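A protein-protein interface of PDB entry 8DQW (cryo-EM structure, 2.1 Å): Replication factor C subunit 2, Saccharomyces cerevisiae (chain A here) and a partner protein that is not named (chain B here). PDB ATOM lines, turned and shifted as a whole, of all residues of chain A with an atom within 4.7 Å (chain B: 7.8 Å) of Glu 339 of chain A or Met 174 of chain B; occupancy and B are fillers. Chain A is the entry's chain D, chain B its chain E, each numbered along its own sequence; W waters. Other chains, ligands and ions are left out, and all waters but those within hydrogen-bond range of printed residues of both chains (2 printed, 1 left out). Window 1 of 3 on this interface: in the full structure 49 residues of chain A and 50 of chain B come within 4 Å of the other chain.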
ATOM      1  N   MET A 291      18.538  -7.924  11.643  1.00  0.00           N
ATOM      2  CA  MET A 291      19.359  -7.259  12.647  1.00  0.00           C
ATOM      3  C   MET A 291      19.811  -5.876  12.201  1.00  0.00           C
ATOM      4  O   MET A 291      20.317  -5.110  13.028  1.00  0.00           O
ATOM      5  CB  MET A 291      20.579  -8.118  12.983  1.00  0.00           C
ATOM      6  CG  MET A 291      20.243  -9.422  13.699  1.00  0.00           C
ATOM      7  SD  MET A 291      19.657  -9.183  15.390  1.00  0.00           S
ATOM      8  CE  MET A 291      21.130  -8.549  16.190  1.00  0.00           C
ATOM      9  N   TRP A 295      16.564  -4.060  16.175  1.00  0.00           N
ATOM     10  CA  TRP A 295      15.602  -4.555  17.151  1.00  0.00           C
ATOM     11  C   TRP A 295      16.326  -5.238  18.305  1.00  0.00           C
ATOM     12  O   TRP A 295      17.330  -5.927  18.108  1.00  0.00           O
ATOM     13  CB  TRP A 295      14.633  -5.539  16.495  1.00  0.00           C
ATOM     14  CG  TRP A 295      13.874  -4.976  15.335  1.00  0.00           C
ATOM     15  CD1 TRP A 295      14.066  -5.262  14.017  1.00  0.00           C
ATOM     16  CD2 TRP A 295      12.794  -4.037  15.389  1.00  0.00           C
ATOM     17  NE1 TRP A 295      13.175  -4.558  13.243  1.00  0.00           N
ATOM     18  CE2 TRP A 295      12.383  -3.798  14.063  1.00  0.00           C
ATOM     19  CE3 TRP A 295      12.135  -3.375  16.429  1.00  0.00           C
ATOM     20  CZ2 TRP A 295      11.345  -2.924  13.750  1.00  0.00           C
ATOM     21  CZ3 TRP A 295      11.105  -2.509  16.116  1.00  0.00           C
ATOM     22  CH2 TRP A 295      10.720  -2.290  14.788  1.00  0.00           C
ATOM     23  N   SER A 296      15.814  -5.041  19.518  1.00  0.00           N
ATOM     24  CA  SER A 296      16.382  -5.691  20.690  1.00  0.00           C
ATOM     25  C   SER A 296      15.933  -7.146  20.734  1.00  0.00           C
ATOM     26  O   SER A 296      14.739  -7.439  20.626  1.00  0.00           O
ATOM     27  CB  SER A 296      15.960  -4.964  21.967  1.00  0.00           C
ATOM     28  OG  SER A 296      14.611  -5.247  22.295  1.00  0.00           O
ATOM     29  N   ALA A 297      16.895  -8.057  20.895  1.00  0.00           N
ATOM     30  CA  ALA A 297      16.580  -9.480  20.839  1.00  0.00           C
ATOM     31  C   ALA A 297      15.614  -9.890  21.941  1.00  0.00           C
ATOM     32  O   ALA A 297      14.818 -10.816  21.752  1.00  0.00           O
ATOM     33  CB  ALA A 297      17.862 -10.307  20.934  1.00  0.00           C
ATOM     34  N   LEU A 333      20.659 -14.454  27.023  1.00  0.00           N
ATOM     35  CA  LEU A 333      20.625 -13.019  26.752  1.00  0.00           C
ATOM     36  C   LEU A 333      20.813 -12.214  28.031  1.00  0.00           C
ATOM     37  O   LEU A 333      21.498 -11.184  28.030  1.00  0.00           O
ATOM     38  CB  LEU A 333      19.310 -12.644  26.070  1.00  0.00           C
ATOM     39  CG  LEU A 333      19.156 -13.076  24.609  1.00  0.00           C
ATOM     40  CD1 LEU A 333      17.752 -12.778  24.113  1.00  0.00           C
ATOM     41  CD2 LEU A 333      20.192 -12.396  23.725  1.00  0.00           C
ATOM     42  N   THR A 337      24.889 -11.621  26.430  1.00  0.00           N
ATOM     43  CA  THR A 337      25.446 -12.337  25.292  1.00  0.00           C
ATOM     44  C   THR A 337      25.199 -11.563  23.998  1.00  0.00           C
ATOM     45  O   THR A 337      24.627 -10.468  23.991  1.00  0.00           O
ATOM     46  CB  THR A 337      24.860 -13.748  25.220  1.00  0.00           C
ATOM     47  OG1 THR A 337      23.445 -13.692  25.429  1.00  0.00           O
ATOM     48  CG2 THR A 337      25.516 -14.667  26.248  1.00  0.00           C
ATOM     49  N   ASN A 338      25.647 -12.134  22.883  1.00  0.00           N
ATOM     50  CA  ASN A 338      25.660 -11.434  21.603  1.00  0.00           C
ATOM     51  C   ASN A 338      24.374 -11.739  20.838  1.00  0.00           C
ATOM     52  O   ASN A 338      24.105 -12.899  20.502  1.00  0.00           O
ATOM     53  CB  ASN A 338      26.896 -11.857  20.811  1.00  0.00           C
ATOM     54  CG  ASN A 338      27.006 -11.163  19.473  1.00  0.00           C
ATOM     55  OD1 ASN A 338      26.289 -11.453  18.520  1.00  0.00           O
ATOM     56  ND2 ASN A 338      27.951 -10.239  19.394  1.00  0.00           N
ATOM     57  N   GLU A 339      23.603 -10.690  20.526  1.00  0.00           N
ATOM     58  CA  GLU A 339      22.196 -10.868  20.160  1.00  0.00           C
ATOM     59  C   GLU A 339      22.022 -11.642  18.854  1.00  0.00           C
ATOM     60  O   GLU A 339      21.148 -12.514  18.759  1.00  0.00           O
ATOM     61  CB  GLU A 339      21.513  -9.505  20.063  1.00  0.00           C
ATOM     62  CG  GLU A 339      21.082  -8.934  21.408  1.00  0.00           C
ATOM     63  CD  GLU A 339      20.728  -7.460  21.340  1.00  0.00           C
ATOM     64  OE1 GLU A 339      19.912  -7.079  20.474  1.00  0.00           O
ATOM     65  OE2 GLU A 339      21.263  -6.681  22.158  1.00  0.00           O
ATOM     66  N   HIS A 340      22.809 -11.318  17.827  1.00  0.00           N
ATOM     67  CA  HIS A 340      22.640 -11.973  16.531  1.00  0.00           C
ATOM     68  C   HIS A 340      22.807 -13.483  16.657  1.00  0.00           C
ATOM     69  O   HIS A 340      21.985 -14.259  16.151  1.00  0.00           O
ATOM     70  CB  HIS A 340      23.648 -11.412  15.526  1.00  0.00           C
ATOM     71  CG  HIS A 340      23.341 -11.744  14.097  1.00  0.00           C
ATOM     72  ND1 HIS A 340      23.715 -10.929  13.050  1.00  0.00           N
ATOM     73  CD2 HIS A 340      22.694 -12.796  13.543  1.00  0.00           C
ATOM     74  CE1 HIS A 340      23.316 -11.469  11.911  1.00  0.00           C
ATOM     75  NE2 HIS A 340      22.693 -12.601  12.183  1.00  0.00           N
ATOM     76  N   ILE A 341      23.875 -13.914  17.329  1.00  0.00           N
ATOM     77  CA  ILE A 341      24.162 -15.340  17.448  1.00  0.00           C
ATOM     78  C   ILE A 341      23.031 -16.047  18.181  1.00  0.00           C
ATOM     79  O   ILE A 341      22.547 -17.100  17.750  1.00  0.00           O
ATOM     80  CB  ILE A 341      25.512 -15.553  18.158  1.00  0.00           C
ATOM     81  CG1 ILE A 341      26.669 -15.165  17.235  1.00  0.00           C
ATOM     82  CG2 ILE A 341      25.655 -17.001  18.610  1.00  0.00           C
ATOM     83  CD1 ILE A 341      27.955 -14.851  17.971  1.00  0.00           C
ATOM     84  N   GLN A 342      22.597 -15.479  19.310  1.00  0.00           N
ATOM     85  CA  GLN A 342      21.553 -16.120  20.103  1.00  0.00           C
ATOM     86  C   GLN A 342      20.246 -16.205  19.327  1.00  0.00           C
ATOM     87  O   GLN A 342      19.570 -17.243  19.346  1.00  0.00           O
ATOM     88  CB  GLN A 342      21.357 -15.362  21.417  1.00  0.00           C
ATOM     89  CG  GLN A 342      22.608 -15.293  22.283  1.00  0.00           C
ATOM     90  CD  GLN A 342      23.107 -16.665  22.705  1.00  0.00           C
ATOM     91  OE1 GLN A 342      22.355 -17.638  22.712  1.00  0.00           O
ATOM     92  NE2 GLN A 342      24.385 -16.746  23.058  1.00  0.00           N
ATOM     93  N   LEU A 343      19.872 -15.127  18.633  1.00  0.00           N
ATOM     94  CA  LEU A 343      18.634 -15.138  17.861  1.00  0.00           C
ATOM     95  C   LEU A 343      18.688 -16.178  16.747  1.00  0.00           C
ATOM     96  O   LEU A 343      17.731 -16.937  16.542  1.00  0.00           O
ATOM     97  CB  LEU A 343      18.364 -13.747  17.282  1.00  0.00           C
ATOM     98  CG  LEU A 343      17.033 -13.562  16.546  1.00  0.00           C
ATOM     99  CD1 LEU A 343      15.866 -14.159  17.327  1.00  0.00           C
ATOM    100  CD2 LEU A 343      16.781 -12.089  16.252  1.00  0.00           C
ATOM    101  N   LEU B  40      18.641   6.696  25.826  1.00  0.00           N
ATOM    102  CA  LEU B  40      19.509   5.559  25.534  1.00  0.00           C
ATOM    103  C   LEU B  40      19.319   5.195  24.067  1.00  0.00           C
ATOM    104  O   LEU B  40      18.278   4.649  23.692  1.00  0.00           O
ATOM    105  CB  LEU B  40      19.190   4.369  26.443  1.00  0.00           C
ATOM    106  CG  LEU B  40      19.925   3.057  26.143  1.00  0.00           C
ATOM    107  CD1 LEU B  40      21.411   3.298  25.944  1.00  0.00           C
ATOM    108  CD2 LEU B  40      19.691   2.041  27.254  1.00  0.00           C
ATOM    109  N   LEU B  41      20.315   5.506  23.244  1.00  0.00           N
ATOM    110  CA  LEU B  41      20.277   5.219  21.816  1.00  0.00           C
ATOM    111  C   LEU B  41      20.981   3.896  21.551  1.00  0.00           C
ATOM    112  O   LEU B  41      22.143   3.720  21.936  1.00  0.00           O
ATOM    113  CB  LEU B  41      20.944   6.340  21.015  1.00  0.00           C
ATOM    114  CG  LEU B  41      20.136   7.629  20.855  1.00  0.00           C
ATOM    115  CD1 LEU B  41      20.257   8.497  22.098  1.00  0.00           C
ATOM    116  CD2 LEU B  41      20.585   8.391  19.616  1.00  0.00           C
ATOM    117  N   TYR B  42      20.280   2.977  20.891  1.00  0.00           N
ATOM    118  CA  TYR B  42      20.815   1.656  20.595  1.00  0.00           C
ATOM    119  C   TYR B  42      20.577   1.304  19.134  1.00  0.00           C
ATOM    120  O   TYR B  42      19.524   1.617  18.572  1.00  0.00           O
ATOM    121  CB  TYR B  42      20.195   0.595  21.517  1.00  0.00           C
ATOM    122  CG  TYR B  42      18.737   0.305  21.249  1.00  0.00           C
ATOM    123  CD1 TYR B  42      17.741   1.057  21.860  1.00  0.00           C
ATOM    124  CD2 TYR B  42      18.353  -0.729  20.406  1.00  0.00           C
ATOM    125  CE1 TYR B  42      16.406   0.797  21.629  1.00  0.00           C
ATOM    126  CE2 TYR B  42      17.019  -0.997  20.168  1.00  0.00           C
ATOM    127  CZ  TYR B  42      16.049  -0.232  20.784  1.00  0.00           C
ATOM    128  OH  TYR B  42      14.718  -0.490  20.553  1.00  0.00           O
ATOM    129  N   GLY B  43      21.569   0.657  18.528  1.00  0.00           N
ATOM    130  CA  GLY B  43      21.491   0.242  17.147  1.00  0.00           C
ATOM    131  C   GLY B  43      22.836  -0.226  16.627  1.00  0.00           C
ATOM    132  O   GLY B  43      23.853  -0.149  17.321  1.00  0.00           O
ATOM    133  N   ASN B 144      27.168  -0.064  26.876  1.00  0.00           N
ATOM    134  CA  ASN B 144      26.997  -1.502  27.050  1.00  0.00           C
ATOM    135  C   ASN B 144      28.223  -2.173  27.656  1.00  0.00           C
ATOM    136  O   ASN B 144      28.112  -3.296  28.157  1.00  0.00           O
ATOM    137  CB  ASN B 144      26.667  -2.152  25.706  1.00  0.00           C
ATOM    138  CG  ASN B 144      27.806  -2.045  24.713  1.00  0.00           C
ATOM    139  OD1 ASN B 144      28.631  -2.951  24.595  1.00  0.00           O
ATOM    140  ND2 ASN B 144      27.860  -0.930  23.996  1.00  0.00           N
ATOM    141  N   GLN B 151      26.942   0.500  36.455  1.00  0.00           N
ATOM    142  CA  GLN B 151      25.543   0.688  36.089  1.00  0.00           C
ATOM    143  C   GLN B 151      24.677   0.872  37.326  1.00  0.00           C
ATOM    144  O   GLN B 151      23.777   1.720  37.343  1.00  0.00           O
ATOM    145  CB  GLN B 151      25.060  -0.500  35.259  1.00  0.00           C
ATOM    146  CG  GLN B 151      25.782  -0.649  33.927  1.00  0.00           C
ATOM    147  CD  GLN B 151      25.090  -1.618  32.992  1.00  0.00           C
ATOM    148  OE1 GLN B 151      23.910  -1.460  32.679  1.00  0.00           O
ATOM    149  NE2 GLN B 151      25.825  -2.623  32.528  1.00  0.00           N
ATOM    150  N   CYS B 171      24.771   2.802  22.833  1.00  0.00           N
ATOM    151  CA  CYS B 171      25.254   1.428  22.837  1.00  0.00           C
ATOM    152  C   CYS B 171      24.930   0.776  21.502  1.00  0.00           C
ATOM    153  O   CYS B 171      24.047   1.223  20.767  1.00  0.00           O
ATOM    154  CB  CYS B 171      24.633   0.610  23.976  1.00  0.00           C
ATOM    155  SG  CYS B 171      22.836   0.717  24.061  1.00  0.00           S
ATOM    156  N   ASP B 172      25.660  -0.297  21.198  1.00  0.00           N
ATOM    157  CA  ASP B 172      25.376  -1.098  20.015  1.00  0.00           C
ATOM    158  C   ASP B 172      24.468  -2.283  20.313  1.00  0.00           C
ATOM    159  O   ASP B 172      23.923  -2.879  19.377  1.00  0.00           O
ATOM    160  CB  ASP B 172      26.680  -1.603  19.384  1.00  0.00           C
ATOM    161  CG  ASP B 172      27.630  -2.206  20.402  1.00  0.00           C
ATOM    162  OD1 ASP B 172      27.158  -2.653  21.469  1.00  0.00           O
ATOM    163  OD2 ASP B 172      28.849  -2.234  20.135  1.00  0.00           O
ATOM    164  N   SER B 173      24.295  -2.634  21.585  1.00  0.00           N
ATOM    165  CA  SER B 173      23.404  -3.715  21.980  1.00  0.00           C
ATOM    166  C   SER B 173      22.961  -3.472  23.415  1.00  0.00           C
ATOM    167  O   SER B 173      23.768  -3.070  24.256  1.00  0.00           O
ATOM    168  CB  SER B 173      24.090  -5.081  21.858  1.00  0.00           C
ATOM    169  OG  SER B 173      25.273  -5.124  22.635  1.00  0.00           O
ATOM    170  N   MET B 174      21.681  -3.716  23.685  1.00  0.00           N
ATOM    171  CA  MET B 174      21.114  -3.498  25.008  1.00  0.00           C
ATOM    172  C   MET B 174      21.132  -4.748  25.879  1.00  0.00           C
ATOM    173  O   MET B 174      20.721  -4.677  27.043  1.00  0.00           O
ATOM    174  CB  MET B 174      19.677  -2.984  24.883  1.00  0.00           C
ATOM    175  CG  MET B 174      19.583  -1.489  24.610  1.00  0.00           C
ATOM    176  SD  MET B 174      17.984  -0.795  25.063  1.00  0.00           S
ATOM    177  CE  MET B 174      16.898  -1.705  23.969  1.00  0.00           C
ATOM    178  N   SER B 175      21.592  -5.884  25.356  1.00  0.00           N
ATOM    179  CA  SER B 175      21.642  -7.093  26.171  1.00  0.00           C
ATOM    180  C   SER B 175      22.456  -6.908  27.447  1.00  0.00           C
ATOM    181  O   SER B 175      22.024  -7.414  28.497  1.00  0.00           O
ATOM    182  CB  SER B 175      22.184  -8.263  25.337  1.00  0.00           C
ATOM    183  OG  SER B 175      23.582  -8.422  25.499  1.00  0.00           O
ATOM    184  N   PRO B 176      23.604  -6.226  27.443  1.00  0.00           N
ATOM    185  CA  PRO B 176      24.381  -6.076  28.681  1.00  0.00           C
ATOM    186  C   PRO B 176      23.887  -4.981  29.617  1.00  0.00           C
ATOM    187  O   PRO B 176      24.474  -4.808  30.691  1.00  0.00           O
ATOM    188  CB  PRO B 176      25.796  -5.747  28.163  1.00  0.00           C
ATOM    189  CG  PRO B 176      25.747  -5.970  26.664  1.00  0.00           C
ATOM    190  CD  PRO B 176      24.339  -5.681  26.293  1.00  0.00           C
ATOM    191  N   ILE B 177      22.846  -4.236  29.256  1.00  0.00           N
ATOM    192  CA  ILE B 177      22.342  -3.166  30.113  1.00  0.00           C
ATOM    193  C   ILE B 177      21.410  -3.762  31.160  1.00  0.00           C
ATOM    194  O   ILE B 177      20.442  -4.454  30.822  1.00  0.00           O
ATOM    195  CB  ILE B 177      21.618  -2.091  29.284  1.00  0.00           C
ATOM    196  CG1 ILE B 177      22.481  -1.628  28.105  1.00  0.00           C
ATOM    197  CG2 ILE B 177      21.237  -0.907  30.169  1.00  0.00           C
ATOM    198  CD1 ILE B 177      23.757  -0.917  28.503  1.00  0.00           C
ATOM    199  N   ILE B 178      21.693  -3.490  32.436  1.00  0.00           N
ATOM    200  CA  ILE B 178      20.853  -4.010  33.506  1.00  0.00           C
ATOM    201  C   ILE B 178      19.460  -3.395  33.412  1.00  0.00           C
ATOM    202  O   ILE B 178      19.278  -2.267  32.934  1.00  0.00           O
ATOM    203  CB  ILE B 178      21.486  -3.748  34.886  1.00  0.00           C
ATOM    204  CG1 ILE B 178      21.614  -2.246  35.160  1.00  0.00           C
ATOM    205  CG2 ILE B 178      22.844  -4.426  34.980  1.00  0.00           C
ATOM    206  CD1 ILE B 178      22.111  -1.925  36.556  1.00  0.00           C
ATOM    207  N   ALA B 179      18.464  -4.150  33.875  1.00  0.00           N
ATOM    208  CA  ALA B 179      17.078  -3.710  33.741  1.00  0.00           C
ATOM    209  C   ALA B 179      16.808  -2.350  34.375  1.00  0.00           C
ATOM    210  O   ALA B 179      16.084  -1.550  33.759  1.00  0.00           O
ATOM    211  CB  ALA B 179      16.144  -4.773  34.333  1.00  0.00           C
ATOM    212  N   LYS B 182      17.769   0.527  31.954  1.00  0.00           N
ATOM    213  CA  LYS B 182      16.810   0.635  30.860  1.00  0.00           C
ATOM    214  C   LYS B 182      15.506   1.256  31.342  1.00  0.00           C
ATOM    215  O   LYS B 182      14.916   2.097  30.653  1.00  0.00           O
ATOM    216  CB  LYS B 182      16.549  -0.741  30.247  1.00  0.00           C
ATOM    217  CG  LYS B 182      17.711  -1.291  29.431  1.00  0.00           C
ATOM    218  CD  LYS B 182      17.464  -2.721  28.953  1.00  0.00           C
ATOM    219  CE  LYS B 182      16.073  -2.907  28.361  1.00  0.00           C
ATOM    220  NZ  LYS B 182      15.973  -4.147  27.541  1.00  0.00           N
ATOM    221  N   CYS B 185      15.411   5.058  31.361  1.00  0.00           N
ATOM    222  CA  CYS B 185      15.795   5.706  30.116  1.00  0.00           C
ATOM    223  C   CYS B 185      14.676   5.636  29.087  1.00  0.00           C
ATOM    224  O   CYS B 185      13.861   4.710  29.084  1.00  0.00           O
ATOM    225  CB  CYS B 185      17.052   5.061  29.521  1.00  0.00           C
ATOM    226  SG  CYS B 185      18.586   5.720  30.175  1.00  0.00           S
ATOM    227  N   LEU B 186      14.654   6.637  28.210  1.00  0.00           N
ATOM    228  CA  LEU B 186      13.863   6.595  26.989  1.00  0.00           C
ATOM    229  C   LEU B 186      14.696   5.904  25.916  1.00  0.00           C
ATOM    230  O   LEU B 186      15.768   6.395  25.546  1.00  0.00           O
ATOM    231  CB  LEU B 186      13.469   8.005  26.551  1.00  0.00           C
ATOM    232  CG  LEU B 186      12.296   8.138  25.574  1.00  0.00           C
ATOM    233  CD1 LEU B 186      11.850   9.589  25.479  1.00  0.00           C
ATOM    234  CD2 LEU B 186      12.655   7.598  24.198  1.00  0.00           C
ATOM    235  N   LEU B 187      14.215   4.761  25.431  1.00  0.00           N
ATOM    236  CA  LEU B 187      14.964   3.943  24.486  1.00  0.00           C
ATOM    237  C   LEU B 187      14.684   4.405  23.062  1.00  0.00           C
ATOM    238  O   LEU B 187      13.523   4.537  22.662  1.00  0.00           O
ATOM    239  CB  LEU B 187      14.600   2.464  24.643  1.00  0.00           C
ATOM    240  CG  LEU B 187      14.327   1.970  26.067  1.00  0.00           C
ATOM    241  CD1 LEU B 187      13.683   0.591  26.045  1.00  0.00           C
ATOM    242  CD2 LEU B 187      15.610   1.954  26.881  1.00  0.00           C
ATOM    243  N   ILE B 188      15.749   4.652  22.303  1.00  0.00           N
ATOM    244  CA  ILE B 188      15.653   5.125  20.928  1.00  0.00           C
ATOM    245  C   ILE B 188      16.396   4.140  20.034  1.00  0.00           C
ATOM    246  O   ILE B 188      17.618   3.976  20.156  1.00  0.00           O
ATOM    247  CB  ILE B 188      16.220   6.545  20.769  1.00  0.00           C
ATOM    248  CG1 ILE B 188      15.464   7.526  21.668  1.00  0.00           C
ATOM    249  CG2 ILE B 188      16.144   6.988  19.312  1.00  0.00           C
ATOM    250  CD1 ILE B 188      16.198   8.831  21.902  1.00  0.00           C
ATOM    251  N   ARG B 189      15.660   3.502  19.131  1.00  0.00           N
ATOM    252  CA  ARG B 189      16.229   2.570  18.168  1.00  0.00           C
ATOM    253  C   ARG B 189      16.717   3.339  16.948  1.00  0.00           C
ATOM    254  O   ARG B 189      15.977   4.147  16.380  1.00  0.00           O
ATOM    255  CB  ARG B 189      15.188   1.527  17.763  1.00  0.00           C
ATOM    256  CG  ARG B 189      15.701   0.463  16.806  1.00  0.00           C
ATOM    257  CD  ARG B 189      14.640  -0.588  16.530  1.00  0.00           C
ATOM    258  NE  ARG B 189      13.404  -0.004  16.020  1.00  0.00           N
ATOM    259  CZ  ARG B 189      13.087   0.101  14.737  1.00  0.00           C
ATOM    260  NH1 ARG B 189      13.900  -0.322  13.783  1.00  0.00           N
ATOM    261  NH2 ARG B 189      11.921   0.646  14.400  1.00  0.00           N
ATOM    262  N   LYS B 301      31.964 -13.748  16.676  1.00  0.00           N
ATOM    263  CA  LYS B 301      30.959 -13.439  15.657  1.00  0.00           C
ATOM    264  C   LYS B 301      31.507 -13.599  14.248  1.00  0.00           C
ATOM    265  O   LYS B 301      30.895 -14.263  13.398  1.00  0.00           O
ATOM    266  CB  LYS B 301      30.434 -12.010  15.803  1.00  0.00           C
ATOM    267  CG  LYS B 301      29.054 -11.846  15.169  1.00  0.00           C
ATOM    268  CD  LYS B 301      28.526 -10.414  15.230  1.00  0.00           C
ATOM    269  CE  LYS B 301      27.023 -10.373  15.240  1.00  0.00           C
ATOM    270  NZ  LYS B 301      26.461 -10.338  16.603  1.00  0.00           N
ATOM    271  N   PHE B 305      30.191 -16.433  11.485  1.00  0.00           N
ATOM    272  CA  PHE B 305      29.435 -16.139  10.273  1.00  0.00           C
ATOM    273  C   PHE B 305      30.260 -16.406   9.019  1.00  0.00           C
ATOM    274  O   PHE B 305      29.705 -16.821   7.990  1.00  0.00           O
ATOM    275  CB  PHE B 305      28.914 -14.705  10.323  1.00  0.00           C
ATOM    276  CG  PHE B 305      27.762 -14.530  11.272  1.00  0.00           C
ATOM    277  CD1 PHE B 305      26.562 -15.186  11.050  1.00  0.00           C
ATOM    278  CD2 PHE B 305      27.886 -13.743  12.402  1.00  0.00           C
ATOM    279  CE1 PHE B 305      25.504 -15.045  11.924  1.00  0.00           C
ATOM    280  CE2 PHE B 305      26.829 -13.598  13.282  1.00  0.00           C
ATOM    281  CZ  PHE B 305      25.639 -14.250  13.042  1.00  0.00           C
ATOM    282  N   ASP B 329      29.840 -18.189  23.211  1.00  0.00           N
ATOM    283  CA  ASP B 329      29.588 -16.776  23.459  1.00  0.00           C
ATOM    284  C   ASP B 329      29.154 -16.551  24.901  1.00  0.00           C
ATOM    285  O   ASP B 329      29.640 -15.628  25.569  1.00  0.00           O
ATOM    286  CB  ASP B 329      28.527 -16.260  22.486  1.00  0.00           C
ATOM    287  CG  ASP B 329      28.306 -14.766  22.602  1.00  0.00           C
ATOM    288  OD1 ASP B 329      29.264 -14.003  22.361  1.00  0.00           O
ATOM    289  OD2 ASP B 329      27.174 -14.355  22.929  1.00  0.00           O
HETATM  290  O   HOH W   1      19.782  -4.347  21.485  1.00  0.00           O
HETATM  291  O   HOH W   2      25.743  -8.117  23.706  1.00  0.00           O
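The side-chain carboxylate (OD2) of Asp 329 of chain B is in hydrogen-bond range of the backbone NH (N) of Asn 338 of chain A (2.7 Å). The backbone carbonyl oxygen (O) of Thr 337 of chain A lies within hydrogen-bond range of the side-chain hydroxyl (OG) of Ser 175 of chain B. The backbone NH (N) of Ser 175 of chain B is in hydrogen-bond range of the side-chain carboxylate (OE2) of Glu 339 of chain A (3.3 Å). The side-chain amide nitrogen (ND2) of Asn 338 of chain A sits close to the side-chain amino group (NZ) of Lys 301 of chain B, at 3.2 Å. The side-chain carboxylate (OE2) of Glu 339 of chain A is in hydrogen-bond range of the backbone NH (N) of Met 174 of chain B (3.4 Å).
N of Ala 297 of chain A sits at hydrogen-bond distance from OE1 of Glu 339 of chain A, at 3.2 Å. The side-chain hydroxyl (OG) of Ser 173 of chain B lies within hydrogen-bond range of the side-chain carboxylate (OD1) of Asp 172 of chain B (3.3 Å). The side-chain hydroxyl (OG1) of Thr 337 of chain A lies close to the backbone NH (N) of Leu 333 of chain A, 3.3 Å away.
Among the printed residues, pairs that only touch across the chains: Trp 295 of chain A with Arg 189 of chain B, Ser 296 of chain A with Met 174 of chain B, Leu 333 of chain A with Ser 175 of chain B, Thr 337 of chain A with Asp 329 of chain B, Glu 339 of chain A with Ser 173 of chain B, His 340 of chain A with Lys 301 of chain B, His 340 of chain A with Phe 305 of chain B and Gln 342 of chain A with Asp 329 of chain B.
Of chain B, only Ser 173, Met 174 and Ser 175 come within 4 Å of Glu 339 of chain A. Of the printed residues of chain A, Met 174 of chain B touches Ser 296 (3.9 Å) and Glu 339 (3.4 Å). Of the printed residues of chain A, Phe 305 of chain B touches His 340 (3.3 Å). Printed residues of chain B within 4 Å of His 340 of chain A: Lys 301 (3.2 Å) and Phe 305 (3.3 Å). Of the printed residues of chain A, Ser 173 of chain B touches Glu 339. Of the printed residues of chain B, Ser 296 of chain A touches Met 174. Of the printed residues of chain A, Arg 189 of chain B touches Trp 295 (3.2 Å). Asn 144 of chain B touches none of the printed residues of chain A. Ile 178 of chain B touches none of the printed residues of chain A. The nearest printed residue of chain A that does not touch Ser 173 of chain B is Thr 337 of chain A (5.6 Å).
Hydrophobic or aromatic side chains of chain B that line the printed part of chain A: Met 174 and Phe 305. Of the 12 printed residues of chain A, 8 touch a printed residue of chain B. Among the printed residues, 13 pairs touch across the chains.
Water W2 lies within hydrogen-bond range of O of Thr 337 of chain A (2.6 Å), OG of Ser 175 of chain B (2.8 Å) and OG of Ser 173 of chain B (3.2 Å). Water W1 bridges OE2 of Glu 339 of chain A (2.8 Å) and N of Met 174 of chain B (3.0 Å).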
